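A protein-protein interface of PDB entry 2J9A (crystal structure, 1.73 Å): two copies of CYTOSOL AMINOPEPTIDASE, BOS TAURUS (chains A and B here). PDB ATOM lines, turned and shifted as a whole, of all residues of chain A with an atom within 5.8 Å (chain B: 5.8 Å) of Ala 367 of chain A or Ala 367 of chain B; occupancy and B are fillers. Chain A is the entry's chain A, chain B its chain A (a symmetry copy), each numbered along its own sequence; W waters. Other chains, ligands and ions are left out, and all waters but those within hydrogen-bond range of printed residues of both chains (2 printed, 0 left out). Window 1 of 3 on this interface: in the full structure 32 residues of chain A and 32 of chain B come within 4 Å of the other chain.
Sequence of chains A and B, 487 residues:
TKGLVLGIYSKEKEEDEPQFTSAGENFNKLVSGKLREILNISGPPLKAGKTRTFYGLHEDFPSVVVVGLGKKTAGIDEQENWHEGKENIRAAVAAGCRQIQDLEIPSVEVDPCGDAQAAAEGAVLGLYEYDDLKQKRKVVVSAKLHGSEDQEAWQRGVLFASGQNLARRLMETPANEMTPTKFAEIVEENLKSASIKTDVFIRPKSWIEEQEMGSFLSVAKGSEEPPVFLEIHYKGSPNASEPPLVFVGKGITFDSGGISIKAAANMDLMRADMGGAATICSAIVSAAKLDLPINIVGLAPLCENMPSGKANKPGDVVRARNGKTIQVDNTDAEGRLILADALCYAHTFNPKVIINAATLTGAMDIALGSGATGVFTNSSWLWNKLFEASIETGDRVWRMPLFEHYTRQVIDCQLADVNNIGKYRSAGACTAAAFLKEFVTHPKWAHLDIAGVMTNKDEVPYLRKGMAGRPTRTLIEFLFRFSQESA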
ATOM      1  N   GLY A 362       3.618 -29.636 -10.477  1.00  0.00           N
ATOM      2  CA  GLY A 362       3.890 -28.218 -10.287  1.00  0.00           C
ATOM      3  C   GLY A 362       4.627 -28.013  -8.984  1.00  0.00           C
ATOM      4  O   GLY A 362       5.452 -27.073  -8.874  1.00  0.00           O
ATOM      5  N   ALA A 363       4.374 -28.892  -8.027  1.00  0.00           N
ATOM      6  CA  ALA A 363       4.996 -28.750  -6.695  1.00  0.00           C
ATOM      7  C   ALA A 363       6.527 -28.839  -6.785  1.00  0.00           C
ATOM      8  O   ALA A 363       7.259 -28.158  -6.050  1.00  0.00           O
ATOM      9  CB  ALA A 363       4.469 -29.820  -5.757  1.00  0.00           C
ATOM     10  N   MET A 364       7.034 -29.652  -7.719  1.00  0.00           N
ATOM     11  CA  MET A 364       8.484 -29.737  -7.882  1.00  0.00           C
ATOM     12  C   MET A 364       9.101 -28.408  -8.327  1.00  0.00           C
ATOM     13  O   MET A 364      10.196 -28.023  -7.858  1.00  0.00           O
ATOM     14  CB  MET A 364       8.870 -30.848  -8.872  1.00  0.00           C
ATOM     15  CG  MET A 364      10.418 -31.024  -9.027  1.00  0.00           C
ATOM     16  SD  MET A 364      11.274 -31.314  -7.436  1.00  0.00           S
ATOM     17  CE  MET A 364      10.649 -32.897  -6.947  1.00  0.00           C
ATOM     18  N   ASP A 365       8.389 -27.697  -9.217  1.00  0.00           N
ATOM     19  CA  ASP A 365       8.857 -26.392  -9.645  1.00  0.00           C
ATOM     20  C   ASP A 365       8.820 -25.396  -8.474  1.00  0.00           C
ATOM     21  O   ASP A 365       9.753 -24.624  -8.254  1.00  0.00           O
ATOM     22  CB  ASP A 365       7.972 -25.840 -10.779  1.00  0.00           C
ATOM     23  CG  ASP A 365       8.483 -24.521 -11.251  1.00  0.00           C
ATOM     24  OD1 ASP A 365       9.654 -24.494 -11.686  1.00  0.00           O
ATOM     25  OD2 ASP A 365       7.814 -23.507 -11.012  1.00  0.00           O
ATOM     26  N   ILE A 366       7.771 -25.474  -7.673  1.00  0.00           N
ATOM     27  CA  ILE A 366       7.723 -24.618  -6.477  1.00  0.00           C
ATOM     28  C   ILE A 366       8.822 -24.977  -5.489  1.00  0.00           C
ATOM     29  O   ILE A 366       9.372 -24.087  -4.869  1.00  0.00           O
ATOM     30  CB  ILE A 366       6.327 -24.707  -5.792  1.00  0.00           C
ATOM     31  CG1 ILE A 366       5.250 -24.192  -6.777  1.00  0.00           C
ATOM     32  CG2 ILE A 366       6.322 -23.893  -4.472  1.00  0.00           C
ATOM     33  CD1 ILE A 366       5.407 -22.745  -7.110  1.00  0.00           C
ATOM     34  N   ALA A 367       9.165 -26.269  -5.374  1.00  0.00           N
ATOM     35  CA  ALA A 367      10.206 -26.712  -4.451  1.00  0.00           C
ATOM     36  C   ALA A 367      11.608 -26.264  -4.853  1.00  0.00           C
ATOM     37  O   ALA A 367      12.325 -25.641  -4.073  1.00  0.00           O
ATOM     38  CB  ALA A 367      10.121 -28.248  -4.334  1.00  0.00           C
ATOM     39  N   LEU A 368      12.046 -26.602  -6.064  1.00  0.00           N
ATOM     40  CA  LEU A 368      13.464 -26.309  -6.434  1.00  0.00           C
ATOM     41  C   LEU A 368      13.608 -25.574  -7.782  1.00  0.00           C
ATOM     42  O   LEU A 368      14.731 -25.223  -8.152  1.00  0.00           O
ATOM     43  CB  LEU A 368      14.255 -27.630  -6.607  1.00  0.00           C
ATOM     44  CG  LEU A 368      14.321 -28.580  -5.395  1.00  0.00           C
ATOM     45  CD1 LEU A 368      15.087 -29.827  -5.759  1.00  0.00           C
ATOM     46  CD2 LEU A 368      15.025 -27.838  -4.253  1.00  0.00           C
ATOM     47  N   GLY A 369      12.500 -25.297  -8.479  1.00  0.00           N
ATOM     48  CA  GLY A 369      12.634 -24.480  -9.716  1.00  0.00           C
ATOM     49  C   GLY A 369      13.556 -25.214 -10.689  1.00  0.00           C
ATOM     50  O   GLY A 369      13.536 -26.440 -10.788  1.00  0.00           O
ATOM     51  N   MET A 400      15.177 -35.885  -2.886  1.00  0.00           N
ATOM     52  CA  MET A 400      13.922 -35.541  -2.233  1.00  0.00           C
ATOM     53  C   MET A 400      13.417 -36.792  -1.550  1.00  0.00           C
ATOM     54  O   MET A 400      13.779 -37.898  -1.930  1.00  0.00           O
ATOM     55  CB  MET A 400      12.915 -35.058  -3.298  1.00  0.00           C
ATOM     56  CG  MET A 400      13.331 -33.747  -3.985  1.00  0.00           C
ATOM     57  SD  MET A 400      13.180 -32.310  -2.885  1.00  0.00           S
ATOM     58  CE  MET A 400      11.396 -32.112  -2.886  1.00  0.00           C
ATOM     59  N   TYR A 406       4.450 -39.720   3.500  1.00  0.00           N
ATOM     60  CA  TYR A 406       3.736 -39.322   2.272  1.00  0.00           C
ATOM     61  C   TYR A 406       2.882 -40.470   1.732  1.00  0.00           C
ATOM     62  O   TYR A 406       1.771 -40.247   1.223  1.00  0.00           O
ATOM     63  CB  TYR A 406       4.778 -38.858   1.245  1.00  0.00           C
ATOM     64  CG  TYR A 406       5.692 -37.748   1.780  1.00  0.00           C
ATOM     65  CD1 TYR A 406       5.170 -36.443   2.040  1.00  0.00           C
ATOM     66  CD2 TYR A 406       7.048 -37.980   2.020  1.00  0.00           C
ATOM     67  CE1 TYR A 406       5.979 -35.417   2.519  1.00  0.00           C
ATOM     68  CE2 TYR A 406       7.906 -36.946   2.507  1.00  0.00           C
ATOM     69  CZ  TYR A 406       7.337 -35.660   2.759  1.00  0.00           C
ATOM     70  OH  TYR A 406       8.171 -34.662   3.240  1.00  0.00           O
ATOM     71  N   ALA A 427       3.461 -30.809  -0.068  1.00  0.00           N
ATOM     72  CA  ALA A 427       4.456 -31.810  -0.498  1.00  0.00           C
ATOM     73  C   ALA A 427       4.022 -32.590  -1.751  1.00  0.00           C
ATOM     74  O   ALA A 427       4.208 -33.814  -1.805  1.00  0.00           O
ATOM     75  CB  ALA A 427       4.809 -32.834   0.655  1.00  0.00           C
ATOM     76  N   GLY A 428       3.466 -31.887  -2.738  1.00  0.00           N
ATOM     77  CA  GLY A 428       2.871 -32.547  -3.898  1.00  0.00           C
ATOM     78  C   GLY A 428       3.858 -33.446  -4.641  1.00  0.00           C
ATOM     79  O   GLY A 428       3.445 -34.459  -5.191  1.00  0.00           O
ATOM     80  N   ALA A 429       5.125 -33.051  -4.719  1.00  0.00           N
ATOM     81  CA  ALA A 429       6.074 -33.883  -5.467  1.00  0.00           C
ATOM     82  C   ALA A 429       6.359 -35.169  -4.658  1.00  0.00           C
ATOM     83  O   ALA A 429       6.667 -36.221  -5.212  1.00  0.00           O
ATOM     84  CB  ALA A 429       7.384 -33.130  -5.694  1.00  0.00           C
ATOM     85  N   CYS A 430       6.289 -35.059  -3.326  1.00  0.00           N
ATOM     86  CA  CYS A 430       6.592 -36.192  -2.438  1.00  0.00           C
ATOM     87  C   CYS A 430       5.474 -37.236  -2.371  1.00  0.00           C
ATOM     88  O   CYS A 430       5.739 -38.465  -2.328  1.00  0.00           O
ATOM     89  CB  CYS A 430       6.902 -35.705  -0.981  1.00  0.00           C
ATOM     90  SG  CYS A 430       8.348 -34.584  -0.876  1.00  0.00           S
ATOM     91  N   GLY B 362       5.517 -20.288   2.102  1.00  0.00           N
ATOM     92  CA  GLY B 362       4.522 -21.272   1.697  1.00  0.00           C
ATOM     93  C   GLY B 362       5.165 -22.305   0.802  1.00  0.00           C
ATOM     94  O   GLY B 362       4.744 -23.489   0.811  1.00  0.00           O
ATOM     95  N   ALA B 363       6.187 -21.890   0.071  1.00  0.00           N
ATOM     96  CA  ALA B 363       6.850 -22.802  -0.880  1.00  0.00           C
ATOM     97  C   ALA B 363       7.472 -24.005  -0.154  1.00  0.00           C
ATOM     98  O   ALA B 363       7.486 -25.135  -0.670  1.00  0.00           O
ATOM     99  CB  ALA B 363       7.919 -22.059  -1.659  1.00  0.00           C
ATOM    100  N   MET B 364       7.959 -23.789   1.073  1.00  0.00           N
ATOM    101  CA  MET B 364       8.516 -24.910   1.829  1.00  0.00           C
ATOM    102  C   MET B 364       7.467 -25.979   2.146  1.00  0.00           C
ATOM    103  O   MET B 364       7.757 -27.196   2.086  1.00  0.00           O
ATOM    104  CB  MET B 364       9.181 -24.429   3.129  1.00  0.00           C
ATOM    105  CG  MET B 364       9.854 -25.587   3.939  1.00  0.00           C
ATOM    106  SD  MET B 364      11.070 -26.542   2.960  1.00  0.00           S
ATOM    107  CE  MET B 364      12.344 -25.348   2.663  1.00  0.00           C
ATOM    108  N   ASP B 365       6.243 -25.528   2.464  1.00  0.00           N
ATOM    109  CA  ASP B 365       5.164 -26.467   2.712  1.00  0.00           C
ATOM    110  C   ASP B 365       4.802 -27.222   1.423  1.00  0.00           C
ATOM    111  O   ASP B 365       4.606 -28.438   1.421  1.00  0.00           O
ATOM    112  CB  ASP B 365       3.906 -25.731   3.213  1.00  0.00           C
ATOM    113  CG  ASP B 365       2.814 -26.703   3.513  1.00  0.00           C
ATOM    114  OD1 ASP B 365       3.061 -27.580   4.367  1.00  0.00           O
ATOM    115  OD2 ASP B 365       1.816 -26.715   2.783  1.00  0.00           O
ATOM    116  N   ILE B 366       4.793 -26.509   0.310  1.00  0.00           N
ATOM    117  CA  ILE B 366       4.552 -27.192  -0.972  1.00  0.00           C
ATOM    118  C   ILE B 366       5.672 -28.166  -1.305  1.00  0.00           C
ATOM    119  O   ILE B 366       5.396 -29.221  -1.844  1.00  0.00           O
ATOM    120  CB  ILE B 366       4.373 -26.157  -2.121  1.00  0.00           C
ATOM    121  CG1 ILE B 366       3.133 -25.282  -1.821  1.00  0.00           C
ATOM    122  CG2 ILE B 366       4.234 -26.884  -3.484  1.00  0.00           C
ATOM    123  CD1 ILE B 366       1.856 -26.056  -1.818  1.00  0.00           C
ATOM    124  N   ALA B 367       6.922 -27.829  -0.949  1.00  0.00           N
ATOM    125  CA  ALA B 367       8.063 -28.697  -1.228  1.00  0.00           C
ATOM    126  C   ALA B 367       8.062 -29.987  -0.413  1.00  0.00           C
ATOM    127  O   ALA B 367       8.137 -31.084  -0.958  1.00  0.00           O
ATOM    128  CB  ALA B 367       9.353 -27.884  -0.989  1.00  0.00           C
ATOM    129  N   LEU B 368       8.015 -29.883   0.914  1.00  0.00           N
ATOM    130  CA  LEU B 368       8.163 -31.116   1.747  1.00  0.00           C
ATOM    131  C   LEU B 368       7.058 -31.274   2.811  1.00  0.00           C
ATOM    132  O   LEU B 368       7.045 -32.291   3.509  1.00  0.00           O
ATOM    133  CB  LEU B 368       9.490 -31.066   2.545  1.00  0.00           C
ATOM    134  CG  LEU B 368      10.798 -30.941   1.739  1.00  0.00           C
ATOM    135  CD1 LEU B 368      11.975 -30.861   2.677  1.00  0.00           C
ATOM    136  CD2 LEU B 368      10.916 -32.178   0.839  1.00  0.00           C
ATOM    137  N   GLY B 369       6.121 -30.323   2.905  1.00  0.00           N
ATOM    138  CA  GLY B 369       4.990 -30.542   3.847  1.00  0.00           C
ATOM    139  C   GLY B 369       5.554 -30.700   5.258  1.00  0.00           C
ATOM    140  O   GLY B 369       6.523 -30.044   5.638  1.00  0.00           O
ATOM    141  N   MET B 400      18.206 -28.600   1.669  1.00  0.00           N
ATOM    142  CA  MET B 400      17.709 -27.891   0.499  1.00  0.00           C
ATOM    143  C   MET B 400      18.832 -27.010  -0.001  1.00  0.00           C
ATOM    144  O   MET B 400      19.733 -26.663   0.752  1.00  0.00           O
ATOM    145  CB  MET B 400      16.489 -27.036   0.908  1.00  0.00           C
ATOM    146  CG  MET B 400      15.280 -27.872   1.360  1.00  0.00           C
ATOM    147  SD  MET B 400      14.479 -28.736  -0.021  1.00  0.00           S
ATOM    148  CE  MET B 400      13.635 -27.356  -0.796  1.00  0.00           C
ATOM    149  N   TYR B 406      19.899 -19.340  -7.384  1.00  0.00           N
ATOM    150  CA  TYR B 406      18.796 -18.647  -6.692  1.00  0.00           C
ATOM    151  C   TYR B 406      19.202 -17.230  -6.285  1.00  0.00           C
ATOM    152  O   TYR B 406      18.386 -16.295  -6.344  1.00  0.00           O
ATOM    153  CB  TYR B 406      18.390 -19.492  -5.477  1.00  0.00           C
ATOM    154  CG  TYR B 406      18.036 -20.938  -5.847  1.00  0.00           C
ATOM    155  CD1 TYR B 406      16.860 -21.225  -6.609  1.00  0.00           C
ATOM    156  CD2 TYR B 406      18.844 -22.006  -5.448  1.00  0.00           C
ATOM    157  CE1 TYR B 406      16.514 -22.527  -6.950  1.00  0.00           C
ATOM    158  CE2 TYR B 406      18.513 -23.355  -5.779  1.00  0.00           C
ATOM    159  CZ  TYR B 406      17.331 -23.591  -6.548  1.00  0.00           C
ATOM    160  OH  TYR B 406      17.018 -24.902  -6.876  1.00  0.00           O
ATOM    161  N   ALA B 427      10.676 -22.118  -6.831  1.00  0.00           N
ATOM    162  CA  ALA B 427      11.710 -22.336  -5.801  1.00  0.00           C
ATOM    163  C   ALA B 427      11.680 -21.278  -4.686  1.00  0.00           C
ATOM    164  O   ALA B 427      12.745 -20.804  -4.262  1.00  0.00           O
ATOM    165  CB  ALA B 427      13.164 -22.397  -6.421  1.00  0.00           C
ATOM    166  N   GLY B 428      10.482 -20.929  -4.217  1.00  0.00           N
ATOM    167  CA  GLY B 428      10.329 -19.819  -3.277  1.00  0.00           C
ATOM    168  C   GLY B 428      11.150 -20.004  -2.001  1.00  0.00           C
ATOM    169  O   GLY B 428      11.607 -19.018  -1.437  1.00  0.00           O
ATOM    170  N   ALA B 429      11.273 -21.234  -1.513  1.00  0.00           N
ATOM    171  CA  ALA B 429      12.020 -21.421  -0.263  1.00  0.00           C
ATOM    172  C   ALA B 429      13.525 -21.211  -0.544  1.00  0.00           C
ATOM    173  O   ALA B 429      14.290 -20.801   0.327  1.00  0.00           O
ATOM    174  CB  ALA B 429      11.803 -22.829   0.286  1.00  0.00           C
ATOM    175  N   CYS B 430      13.951 -21.534  -1.772  1.00  0.00           N
ATOM    176  CA  CYS B 430      15.369 -21.434  -2.151  1.00  0.00           C
ATOM    177  C   CYS B 430      15.835 -19.998  -2.410  1.00  0.00           C
ATOM    178  O   CYS B 430      16.973 -19.611  -2.039  1.00  0.00           O
ATOM    179  CB  CYS B 430      15.677 -22.292  -3.425  1.00  0.00           C
ATOM    180  SG  CYS B 430      15.342 -24.079  -3.202  1.00  0.00           S
HETATM  181  O   HOH W   1      10.838 -23.846  -2.606  1.00  0.00           O
HETATM  182  O   HOH W   2       6.679 -31.112  -3.296  1.00  0.00           O
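The side-chain hydroxyl (OH) of Tyr 406 of chain A sits at hydrogen-bond distance from the backbone carbonyl oxygen (O) of Leu 368 of chain B (2.6 Å). The backbone carbonyl oxygen (O) of Leu 368 of chain A lies within hydrogen-bond range of the side-chain hydroxyl (OH) of Tyr 406 of chain B (2.6 Å). The backbone NH (N) of Ala 427 of chain A sits at hydrogen-bond distance from the backbone carbonyl oxygen (O) of Asp 365 of chain B, at 3.0 Å. O of Ile 366 of chain A is in hydrogen-bond range of N of Gly 428 of chain B (3.4 Å). The backbone NH of Ala 427 of chain B lies close to the backbone carbonyl oxygen of Ile 366 of chain A (3.1 Å). N of Ala 427 of chain B sits at hydrogen-bond distance from O of Asp 365 of chain A (3.0 Å). O of Ile 366 of chain B lies close to N of Ala 427 of chain A, at 3.1 Å. The side-chain sulfur of Cys 430 of chain A sits at hydrogen-bond distance from the backbone carbonyl oxygen of Ala 367 of chain B (3.5 Å). The backbone carbonyl oxygen (O) of Ala 367 of chain A lies within hydrogen-bond range of the side-chain sulfur (SG) of Cys 430 of chain B (3.5 Å). O of Ile 366 of chain B is in hydrogen-bond range of N of Gly 428 of chain A, at 3.4 Å.
Ile 366 of chain B touches Ala 363 of chain A. CG2 of Ile 366 of chain A touches CG2 of Ile 366 of chain B, at 3.8 Å. CB of Ala 367 of chain B touches CB of Ala 367 of chain A (3.5 Å). CD2 of Leu 368 of chain A touches CE of Met 400 of chain B, 3.8 Å away. C of Leu 368 of chain A touches CB of Ala 427 of chain B, at 3.5 Å. Cys 430 of chain B touches Leu 368 of chain A. Met 400 of chain A touches Leu 368 of chain B. CB of Ala 427 of chain A touches C of Leu 368 of chain B (3.5 Å). Gly 369 of chain B touches Ala 427 of chain A. Cys 430 of chain A touches Leu 368 of chain B (SG to CD2, 3.9 Å).
Of chain B, only Ala 367, Met 400, Ala 427 and Cys 430 come within 4 Å of Ala 367 of chain A. Ala 367 of chain B touches just these residues of chain A: Ala 367 (3.5 Å), Met 400 (3.9 Å), Ala 427 (3.8 Å) and Cys 430 (3.5 Å). Printed residues of chain A within 4 Å of Ile 366 of chain B: Ala 363, Ile 366, Ala 427 and Gly 428. Of the printed residues of chain A, Ala 363 of chain B touches Ile 366. The nearest printed residue of chain B that does not touch Tyr 406 of chain A is Gly 369 of chain B (4.8 Å).
Hydrophobic or aromatic side chains of chain A that line the printed part of chain B: Ala 363, Ile 366, Ala 367, Leu 368, Met 400, Tyr 406 and Ala 427. Among the printed residues, 26 pairs touch across the chains.
Ile 366 of chain B touches its own counterpart, Ile 366 of chain A. Ala 367 of chain A touches Cys 430 of chain B, and with the chains exchanged Cys 430 of chain A touches Ala 367 of chain B. Leu 368 of chain A touches Met 400 of chain B, and with the chains exchanged Met 400 of chain A touches Leu 368 of chain B. Leu 368 of chain A touches Tyr 406 of chain B, and with the chains exchanged Tyr 406 of chain A touches Leu 368 of chain B.
Water W1 lies within hydrogen-bond range of O of Ile 366 of chain A, O of Ala 367 of chain A, N of Ala 429 of chain B and N of Gly 428 of chain B. Water W2 lies within hydrogen-bond range of O of Ile 366 of chain B, O of Ala 367 of chain B, N of Ala 429 of chain A and N of Gly 428 of chain A.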
